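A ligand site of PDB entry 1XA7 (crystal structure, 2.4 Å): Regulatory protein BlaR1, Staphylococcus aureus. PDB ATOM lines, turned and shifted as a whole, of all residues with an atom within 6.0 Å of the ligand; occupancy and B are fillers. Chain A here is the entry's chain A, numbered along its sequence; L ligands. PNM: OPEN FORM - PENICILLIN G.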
ATOM      1  N   PRO A  57      -2.213  -9.673  13.426  1.00  0.00           N
ATOM      2  CA  PRO A  57      -1.132  -8.680  13.332  1.00  0.00           C
ATOM      3  C   PRO A  57       0.210  -9.360  13.108  1.00  0.00           C
ATOM      4  O   PRO A  57       1.209  -8.691  12.869  1.00  0.00           O
ATOM      5  CB  PRO A  57      -1.141  -8.033  14.727  1.00  0.00           C
ATOM      6  CG  PRO A  57      -1.458  -9.167  15.641  1.00  0.00           C
ATOM      7  CD  PRO A  57      -2.499  -9.993  14.839  1.00  0.00           C
ATOM      8  N   ASN A  58       0.216 -10.674  13.187  1.00  0.00           N
ATOM      9  CA  ASN A  58       1.438 -11.456  13.275  1.00  0.00           C
ATOM     10  C   ASN A  58       2.610 -10.681  13.913  1.00  0.00           C
ATOM     11  O   ASN A  58       2.453 -10.264  15.072  1.00  0.00           O
ATOM     12  CB  ASN A  58       1.759 -12.263  11.972  1.00  0.00           C
ATOM     13  CG  ASN A  58       1.573 -11.458  10.725  1.00  0.00           C
ATOM     14  OD1 ASN A  58       2.322 -10.510  10.495  1.00  0.00           O
ATOM     15  ND2 ASN A  58       0.599 -11.862   9.884  1.00  0.00           N
ATOM     16  N   SER A  59       3.747 -10.505  13.222  1.00  0.00           N
ATOM     17  CA  SER A  59       4.948  -9.966  13.861  1.00  0.00           C
ATOM     18  C   SER A  59       4.848  -8.516  14.229  1.00  0.00           C
ATOM     19  O   SER A  59       5.773  -8.138  15.182  1.00  0.00           O
ATOM     20  CB  SER A  59       6.221 -10.175  13.060  1.00  0.00           C
ATOM     21  OG  SER A  59       6.428 -11.570  13.043  1.00  0.00           O
ATOM     22  N   THR A  60       3.922  -7.712  13.701  1.00  0.00           N
ATOM     23  CA  THR A  60       3.687  -6.375  14.252  1.00  0.00           C
ATOM     24  C   THR A  60       3.280  -6.375  15.736  1.00  0.00           C
ATOM     25  O   THR A  60       3.325  -5.326  16.390  1.00  0.00           O
ATOM     26  CB  THR A  60       2.642  -5.585  13.417  1.00  0.00           C
ATOM     27  OG1 THR A  60       1.314  -6.141  13.575  1.00  0.00           O
ATOM     28  CG2 THR A  60       2.965  -5.633  11.914  1.00  0.00           C
ATOM     29  N   LYS A  62       4.842  -7.811  17.999  1.00  0.00           N
ATOM     30  CA  LYS A  62       6.060  -7.776  18.747  1.00  0.00           C
ATOM     31  C   LYS A  62       6.240  -6.415  19.396  1.00  0.00           C
ATOM     32  O   LYS A  62       6.805  -6.310  20.479  1.00  0.00           O
ATOM     33  CB  LYS A  62       7.230  -8.151  17.858  1.00  0.00           C
ATOM     34  CG  LYS A  62       7.198  -9.686  17.419  1.00  0.00           C
ATOM     35  CD  LYS A  62       8.322  -9.999  16.418  1.00  0.00           C
ATOM     36  CE  LYS A  62       8.377 -11.484  16.034  1.00  0.00           C
ATOM     37  NZ  LYS A  62       9.519 -11.911  15.162  1.00  0.00           N
ATOM     38  N   PHE A  91      16.547 -18.743   9.412  1.00  0.00           N
ATOM     39  CA  PHE A  91      17.242 -17.465   9.445  1.00  0.00           C
ATOM     40  C   PHE A  91      18.512 -17.585  10.289  1.00  0.00           C
ATOM     41  O   PHE A  91      18.464 -17.934  11.449  1.00  0.00           O
ATOM     42  CB  PHE A  91      16.344 -16.381  10.050  1.00  0.00           C
ATOM     43  CG  PHE A  91      14.953 -16.269   9.422  1.00  0.00           C
ATOM     44  CD1 PHE A  91      13.867 -16.967   9.984  1.00  0.00           C
ATOM     45  CD2 PHE A  91      14.730 -15.438   8.318  1.00  0.00           C
ATOM     46  CE1 PHE A  91      12.572 -16.842   9.430  1.00  0.00           C
ATOM     47  CE2 PHE A  91      13.425 -15.319   7.756  1.00  0.00           C
ATOM     48  CZ  PHE A  91      12.358 -16.027   8.315  1.00  0.00           C
ATOM     49  N   TRP A  94      18.620 -15.278  13.583  1.00  0.00           N
ATOM     50  CA  TRP A  94      17.964 -15.921  14.736  1.00  0.00           C
ATOM     51  C   TRP A  94      18.874 -16.856  15.586  1.00  0.00           C
ATOM     52  O   TRP A  94      18.490 -17.279  16.690  1.00  0.00           O
ATOM     53  CB  TRP A  94      16.760 -16.774  14.247  1.00  0.00           C
ATOM     54  CG  TRP A  94      15.575 -15.989  13.690  1.00  0.00           C
ATOM     55  CD1 TRP A  94      15.578 -14.688  13.256  1.00  0.00           C
ATOM     56  CD2 TRP A  94      14.243 -16.474  13.487  1.00  0.00           C
ATOM     57  NE1 TRP A  94      14.336 -14.349  12.799  1.00  0.00           N
ATOM     58  CE2 TRP A  94      13.500 -15.415  12.931  1.00  0.00           C
ATOM     59  CE3 TRP A  94      13.607 -17.700  13.713  1.00  0.00           C
ATOM     60  CZ2 TRP A  94      12.154 -15.544  12.601  1.00  0.00           C
ATOM     61  CZ3 TRP A  94      12.263 -17.839  13.391  1.00  0.00           C
ATOM     62  CH2 TRP A  94      11.543 -16.758  12.850  1.00  0.00           C
ATOM     63  N   ASN A 106      15.468  -8.059  13.450  1.00  0.00           N
ATOM     64  CA  ASN A 106      15.548  -9.348  12.782  1.00  0.00           C
ATOM     65  C   ASN A 106      14.329 -10.244  13.020  1.00  0.00           C
ATOM     66  O   ASN A 106      14.318 -11.415  12.693  1.00  0.00           O
ATOM     67  CB  ASN A 106      16.819 -10.024  13.238  1.00  0.00           C
ATOM     68  CG  ASN A 106      18.055  -9.366  12.663  1.00  0.00           C
ATOM     69  OD1 ASN A 106      18.060  -9.064  11.482  1.00  0.00           O
ATOM     70  ND2 ASN A 106      19.091  -9.139  13.475  1.00  0.00           N
ATOM     71  N   SER A 107      13.300  -9.643  13.592  1.00  0.00           N
ATOM     72  CA  SER A 107      12.041 -10.307  13.835  1.00  0.00           C
ATOM     73  C   SER A 107      12.205 -11.744  14.305  1.00  0.00           C
ATOM     74  O   SER A 107      11.665 -12.659  13.712  1.00  0.00           O
ATOM     75  CB  SER A 107      11.173 -10.227  12.586  1.00  0.00           C
ATOM     76  OG  SER A 107       9.840 -10.482  12.917  1.00  0.00           O
ATOM     77  N   ASN A 109      11.319 -14.626  16.294  1.00  0.00           N
ATOM     78  CA  ASN A 109      10.128 -15.123  16.957  1.00  0.00           C
ATOM     79  C   ASN A 109      10.418 -15.716  18.329  1.00  0.00           C
ATOM     80  O   ASN A 109       9.661 -15.474  19.262  1.00  0.00           O
ATOM     81  CB  ASN A 109       9.394 -16.158  16.102  1.00  0.00           C
ATOM     82  CG  ASN A 109       8.643 -15.517  14.954  1.00  0.00           C
ATOM     83  OD1 ASN A 109       8.371 -14.324  14.971  1.00  0.00           O
ATOM     84  ND2 ASN A 109       8.292 -16.301  13.960  1.00  0.00           N
ATOM     85  N   MET A 146       0.032 -14.876  16.107  1.00  0.00           N
ATOM     86  CA  MET A 146       0.536 -15.502  14.842  1.00  0.00           C
ATOM     87  C   MET A 146      -0.594 -16.238  14.077  1.00  0.00           C
ATOM     88  O   MET A 146      -0.783 -17.406  14.265  1.00  0.00           O
ATOM     89  CB  MET A 146       1.718 -16.454  15.146  1.00  0.00           C
ATOM     90  CG  MET A 146       2.936 -15.779  15.786  1.00  0.00           C
ATOM     91  SD  MET A 146       3.791 -14.504  14.513  1.00  0.00           S
ATOM     92  CE  MET A 146       5.287 -15.700  14.167  1.00  0.00           C
ATOM     93  N   GLU A 147      -1.336 -15.529  13.238  1.00  0.00           N
ATOM     94  CA  GLU A 147      -2.475 -16.072  12.457  1.00  0.00           C
ATOM     95  C   GLU A 147      -3.342 -16.941  13.294  1.00  0.00           C
ATOM     96  O   GLU A 147      -3.252 -18.183  13.188  1.00  0.00           O
ATOM     97  CB  GLU A 147      -2.015 -16.875  11.235  1.00  0.00           C
ATOM     98  CG  GLU A 147      -1.201 -16.091  10.200  1.00  0.00           C
ATOM     99  CD  GLU A 147      -1.906 -14.889   9.546  1.00  0.00           C
ATOM    100  OE1 GLU A 147      -1.231 -13.868   9.399  1.00  0.00           O
ATOM    101  OE2 GLU A 147      -3.087 -14.958   9.122  1.00  0.00           O
ATOM    102  N   LYS A 196       7.670  -1.780  11.977  1.00  0.00           N
ATOM    103  CA  LYS A 196       7.823  -3.185  12.105  1.00  0.00           C
ATOM    104  C   LYS A 196       7.047  -3.924  10.990  1.00  0.00           C
ATOM    105  O   LYS A 196       5.886  -3.603  10.746  1.00  0.00           O
ATOM    106  CB  LYS A 196       7.351  -3.605  13.493  1.00  0.00           C
ATOM    107  CG  LYS A 196       7.491  -5.030  13.772  1.00  0.00           C
ATOM    108  CD  LYS A 196       8.942  -5.431  13.911  1.00  0.00           C
ATOM    109  CE  LYS A 196       9.055  -6.918  14.043  1.00  0.00           C
ATOM    110  NZ  LYS A 196       9.254  -7.522  12.681  1.00  0.00           N
ATOM    111  N   THR A 197       7.725  -4.859  10.326  1.00  0.00           N
ATOM    112  CA  THR A 197       7.138  -5.719   9.297  1.00  0.00           C
ATOM    113  C   THR A 197       6.393  -6.883   9.897  1.00  0.00           C
ATOM    114  O   THR A 197       6.677  -7.320  11.007  1.00  0.00           O
ATOM    115  CB  THR A 197       8.200  -6.333   8.365  1.00  0.00           C
ATOM    116  OG1 THR A 197       9.303  -6.876   9.143  1.00  0.00           O
ATOM    117  CG2 THR A 197       8.814  -5.324   7.416  1.00  0.00           C
ATOM    118  N   GLY A 198       5.407  -7.353   9.169  1.00  0.00           N
ATOM    119  CA  GLY A 198       4.649  -8.522   9.567  1.00  0.00           C
ATOM    120  C   GLY A 198       4.464  -9.356   8.312  1.00  0.00           C
ATOM    121  O   GLY A 198       4.174  -8.770   7.235  1.00  0.00           O
ATOM    122  N   THR A 199       4.655 -10.669   8.428  1.00  0.00           N
ATOM    123  CA  THR A 199       4.401 -11.553   7.292  1.00  0.00           C
ATOM    124  C   THR A 199       3.723 -12.837   7.727  1.00  0.00           C
ATOM    125  O   THR A 199       4.316 -13.647   8.415  1.00  0.00           O
ATOM    126  CB  THR A 199       5.705 -11.876   6.500  1.00  0.00           C
ATOM    127  OG1 THR A 199       6.289 -10.672   6.019  1.00  0.00           O
ATOM    128  CG2 THR A 199       5.421 -12.664   5.214  1.00  0.00           C
ATOM    129  N   GLY A 200       2.505 -13.034   7.255  1.00  0.00           N
ATOM    130  CA  GLY A 200       1.684 -14.172   7.642  1.00  0.00           C
ATOM    131  C   GLY A 200       1.838 -15.282   6.639  1.00  0.00           C
ATOM    132  O   GLY A 200       1.993 -15.020   5.446  1.00  0.00           O
ATOM    133  N   ILE A 201       1.844 -16.507   7.138  1.00  0.00           N
ATOM    134  CA  ILE A 201       1.661 -17.730   6.343  1.00  0.00           C
ATOM    135  C   ILE A 201       0.767 -18.678   7.115  1.00  0.00           C
ATOM    136  O   ILE A 201      -0.271 -19.078   6.602  1.00  0.00           O
ATOM    137  CB  ILE A 201       3.035 -18.403   5.915  1.00  0.00           C
ATOM    138  CG1 ILE A 201       3.009 -19.951   6.123  1.00  0.00           C
ATOM    139  CG2 ILE A 201       4.238 -17.763   6.593  1.00  0.00           C
ATOM    140  CD1 ILE A 201       3.318 -20.446   7.609  1.00  0.00           C
ATOM    141  N   TYR A 206       1.763 -17.071   1.649  1.00  0.00           N
ATOM    142  CA  TYR A 206       1.800 -15.683   2.106  1.00  0.00           C
ATOM    143  C   TYR A 206       0.434 -15.038   1.879  1.00  0.00           C
ATOM    144  O   TYR A 206       0.020 -14.918   0.731  1.00  0.00           O
ATOM    145  CB  TYR A 206       2.858 -14.881   1.357  1.00  0.00           C
ATOM    146  CG  TYR A 206       4.301 -15.213   1.680  1.00  0.00           C
ATOM    147  CD1 TYR A 206       4.633 -16.255   2.542  1.00  0.00           C
ATOM    148  CD2 TYR A 206       5.348 -14.498   1.075  1.00  0.00           C
ATOM    149  CE1 TYR A 206       5.957 -16.563   2.840  1.00  0.00           C
ATOM    150  CE2 TYR A 206       6.692 -14.807   1.348  1.00  0.00           C
ATOM    151  CZ  TYR A 206       6.996 -15.844   2.241  1.00  0.00           C
ATOM    152  OH  TYR A 206       8.315 -16.172   2.563  1.00  0.00           O
ATOM    153  N   TRP A 210       2.240  -6.738   6.486  1.00  0.00           N
ATOM    154  CA  TRP A 210       2.037  -5.505   7.246  1.00  0.00           C
ATOM    155  C   TRP A 210       3.298  -4.703   7.325  1.00  0.00           C
ATOM    156  O   TRP A 210       4.375  -5.260   7.399  1.00  0.00           O
ATOM    157  CB  TRP A 210       1.777  -5.825   8.692  1.00  0.00           C
ATOM    158  CG  TRP A 210       0.547  -6.396   9.064  1.00  0.00           C
ATOM    159  CD1 TRP A 210       0.329  -7.685   9.448  1.00  0.00           C
ATOM    160  CD2 TRP A 210      -0.659  -5.693   9.301  1.00  0.00           C
ATOM    161  NE1 TRP A 210      -0.980  -7.848   9.850  1.00  0.00           N
ATOM    162  CE2 TRP A 210      -1.606  -6.631   9.779  1.00  0.00           C
ATOM    163  CE3 TRP A 210      -1.052  -4.372   9.139  1.00  0.00           C
ATOM    164  CZ2 TRP A 210      -2.913  -6.276  10.086  1.00  0.00           C
ATOM    165  CZ3 TRP A 210      -2.331  -4.043   9.446  1.00  0.00           C
ATOM    166  CH2 TRP A 210      -3.242  -4.987   9.921  1.00  0.00           C
ATOM    167  N   SER A 234       3.418  -9.449   1.562  1.00  0.00           N
ATOM    168  CA  SER A 234       4.662  -9.741   2.265  1.00  0.00           C
ATOM    169  C   SER A 234       5.025  -8.515   3.088  1.00  0.00           C
ATOM    170  O   SER A 234       4.706  -7.385   2.748  1.00  0.00           O
ATOM    171  CB  SER A 234       5.747 -10.203   1.261  1.00  0.00           C
ATOM    172  OG  SER A 234       6.741  -9.223   0.949  1.00  0.00           O
ATOM    173  N   GLY A 235       5.665  -8.769   4.207  1.00  0.00           N
ATOM    174  CA  GLY A 235       6.126  -7.700   5.081  1.00  0.00           C
ATOM    175  C   GLY A 235       7.012  -6.793   4.292  1.00  0.00           C
ATOM    176  O   GLY A 235       6.880  -5.565   4.373  1.00  0.00           O
ATOM    177  N   LYS A 236       7.911  -7.408   3.519  1.00  0.00           N
ATOM    178  CA  LYS A 236       8.820  -6.675   2.616  1.00  0.00           C
ATOM    179  C   LYS A 236       8.096  -5.748   1.640  1.00  0.00           C
ATOM    180  O   LYS A 236       8.493  -4.589   1.507  1.00  0.00           O
ATOM    181  CB  LYS A 236       9.770  -7.626   1.851  1.00  0.00           C
ATOM    182  CG  LYS A 236      11.086  -6.921   1.446  1.00  0.00           C
ATOM    183  CD  LYS A 236      11.954  -7.699   0.451  1.00  0.00           C
ATOM    184  CE  LYS A 236      11.606  -7.338  -0.995  1.00  0.00           C
ATOM    185  NZ  LYS A 236      10.109  -7.128  -1.168  1.00  0.00           N
HETATM  186  O8  PNM L   1       5.404 -11.800  11.036  1.00  0.00           O
HETATM  187  C7  PNM L   1       6.206 -12.274  11.812  1.00  0.00           C
HETATM  188  N4  PNM L   1       8.059 -11.717  10.400  1.00  0.00           N
HETATM  189  C3  PNM L   1       8.345 -11.586   9.008  1.00  0.00           C
HETATM  190  C11 PNM L   1       8.548 -10.132   8.667  1.00  0.00           C
HETATM  191  O13 PNM L   1       7.985  -9.689   7.623  1.00  0.00           O
HETATM  192  O12 PNM L   1       9.228  -9.441   9.476  1.00  0.00           O
HETATM  193  C2  PNM L   1       9.328 -12.705   8.546  1.00  0.00           C
HETATM  194  C10 PNM L   1      10.708 -12.052   8.355  1.00  0.00           C
HETATM  195  C9  PNM L   1       8.942 -13.463   7.287  1.00  0.00           C
HETATM  196  S1  PNM L   1       9.387 -13.854   9.896  1.00  0.00           S
HETATM  197  C5  PNM L   1       8.421 -12.928  11.084  1.00  0.00           C
HETATM  198  C6  PNM L   1       7.040 -13.457  11.483  1.00  0.00           C
HETATM  199  N14 PNM L   1       6.369 -14.242  10.457  1.00  0.00           N
HETATM  200  C15 PNM L   1       6.472 -15.553  10.446  1.00  0.00           C
HETATM  201  O16 PNM L   1       7.184 -16.093  11.240  1.00  0.00           O
HETATM  202  C17 PNM L   1       5.636 -16.356   9.452  1.00  0.00           C
HETATM  203  C18 PNM L   1       4.449 -16.938  10.225  1.00  0.00           C
HETATM  204  C19 PNM L   1       3.369 -16.122  10.594  1.00  0.00           C
HETATM  205  C20 PNM L   1       2.297 -16.662  11.326  1.00  0.00           C
HETATM  206  C21 PNM L   1       2.314 -18.010  11.697  1.00  0.00           C
HETATM  207  C22 PNM L   1       3.406 -18.821  11.321  1.00  0.00           C
HETATM  208  C23 PNM L   1       4.457 -18.293  10.588  1.00  0.00           C
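CE of Met 146 touches O16 of the ligand, 3.5 Å away.
Glu 147 touches the ligand (CG to C20, 3.7 Å).
C of Gly 198 touches O13 of the ligand (3.6 Å).
Gly 200 touches the ligand (CA to C19, 3.9 Å).
CG2 of Ile 201 touches C17 of the ligand, 3.5 Å away.
Gly 235 touches the ligand (CA to O13, 3.7 Å).
Hydrophobic or aromatic side chains that line the ligand: Met 146 and Ile 201.
13 residues have an atom within 4 Å of the ligand: Asn 58, Ser 59, Ser 107, Asn 109, Met 146, Glu 147, Lys 196, Thr 197, Gly 198, Thr 199, Gly 200, Ile 201 and Gly 235.
The backbone carbonyl oxygen (O) of Gly 198 lies within hydrogen-bond range of the backbone NH (N) of Trp 210.
The backbone NH (N) of Thr 199 lies within hydrogen-bond range of the side-chain amide oxygen (OD1) of Asn 58 (3.1 Å).
The indole nitrogen (NE1) of Trp 94 sits close to the backbone carbonyl oxygen (O) of Ser 107 (3.3 Å).
The backbone NH (N) of Gly 235 lies close to the backbone carbonyl oxygen (O) of Gly 198, at 3.4 Å.
The side-chain hydroxyl of Ser 107 sits at hydrogen-bond distance from the side-chain amino group of Lys 62, 2.7 Å away.
The side-chain hydroxyl (OG) of Ser 107 is in hydrogen-bond range of the side-chain amino group (NZ) of Lys 196, at 3.0 Å.
The side-chain amino group (NZ) of Lys 62 is in hydrogen-bond range of the side-chain amide oxygen (OD1) of Asn 109, 2.7 Å away.
N of Gly 200 sits close to ND2 of Asn 58 (3.5 Å).
The backbone NH (N) of Ser 59 lies close to an oxygen (O8) of the ligand, at 3.0 Å.
N14 of the ligand lies within hydrogen-bond range of O of Thr 199.
OD1 of Asn 58 lies close to O8 of the ligand, at 3.4 Å.
The side-chain hydroxyl (OG1) of Thr 199 is in hydrogen-bond range of an oxygen (O13) of the ligand (2.5 Å).
NZ of Lys 196 is in salt-bridge range of O12 of the ligand (3.7 Å).
OG of Ser 59 is covalently linked to C7 of the ligand (1.4 Å).
O8 of the ligand sits at hydrogen-bond distance from N of Thr 199 (2.9 Å).
ND2 of Asn 109 is in hydrogen-bond range of O16 of the ligand.
The side-chain hydroxyl (OG1) of Thr 197 lies within hydrogen-bond range of an oxygen (O12) of the ligand.
A nitrogen (N4) of the ligand lies within hydrogen-bond range of the side-chain hydroxyl (OG) of Ser 107, at 3.3 Å.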
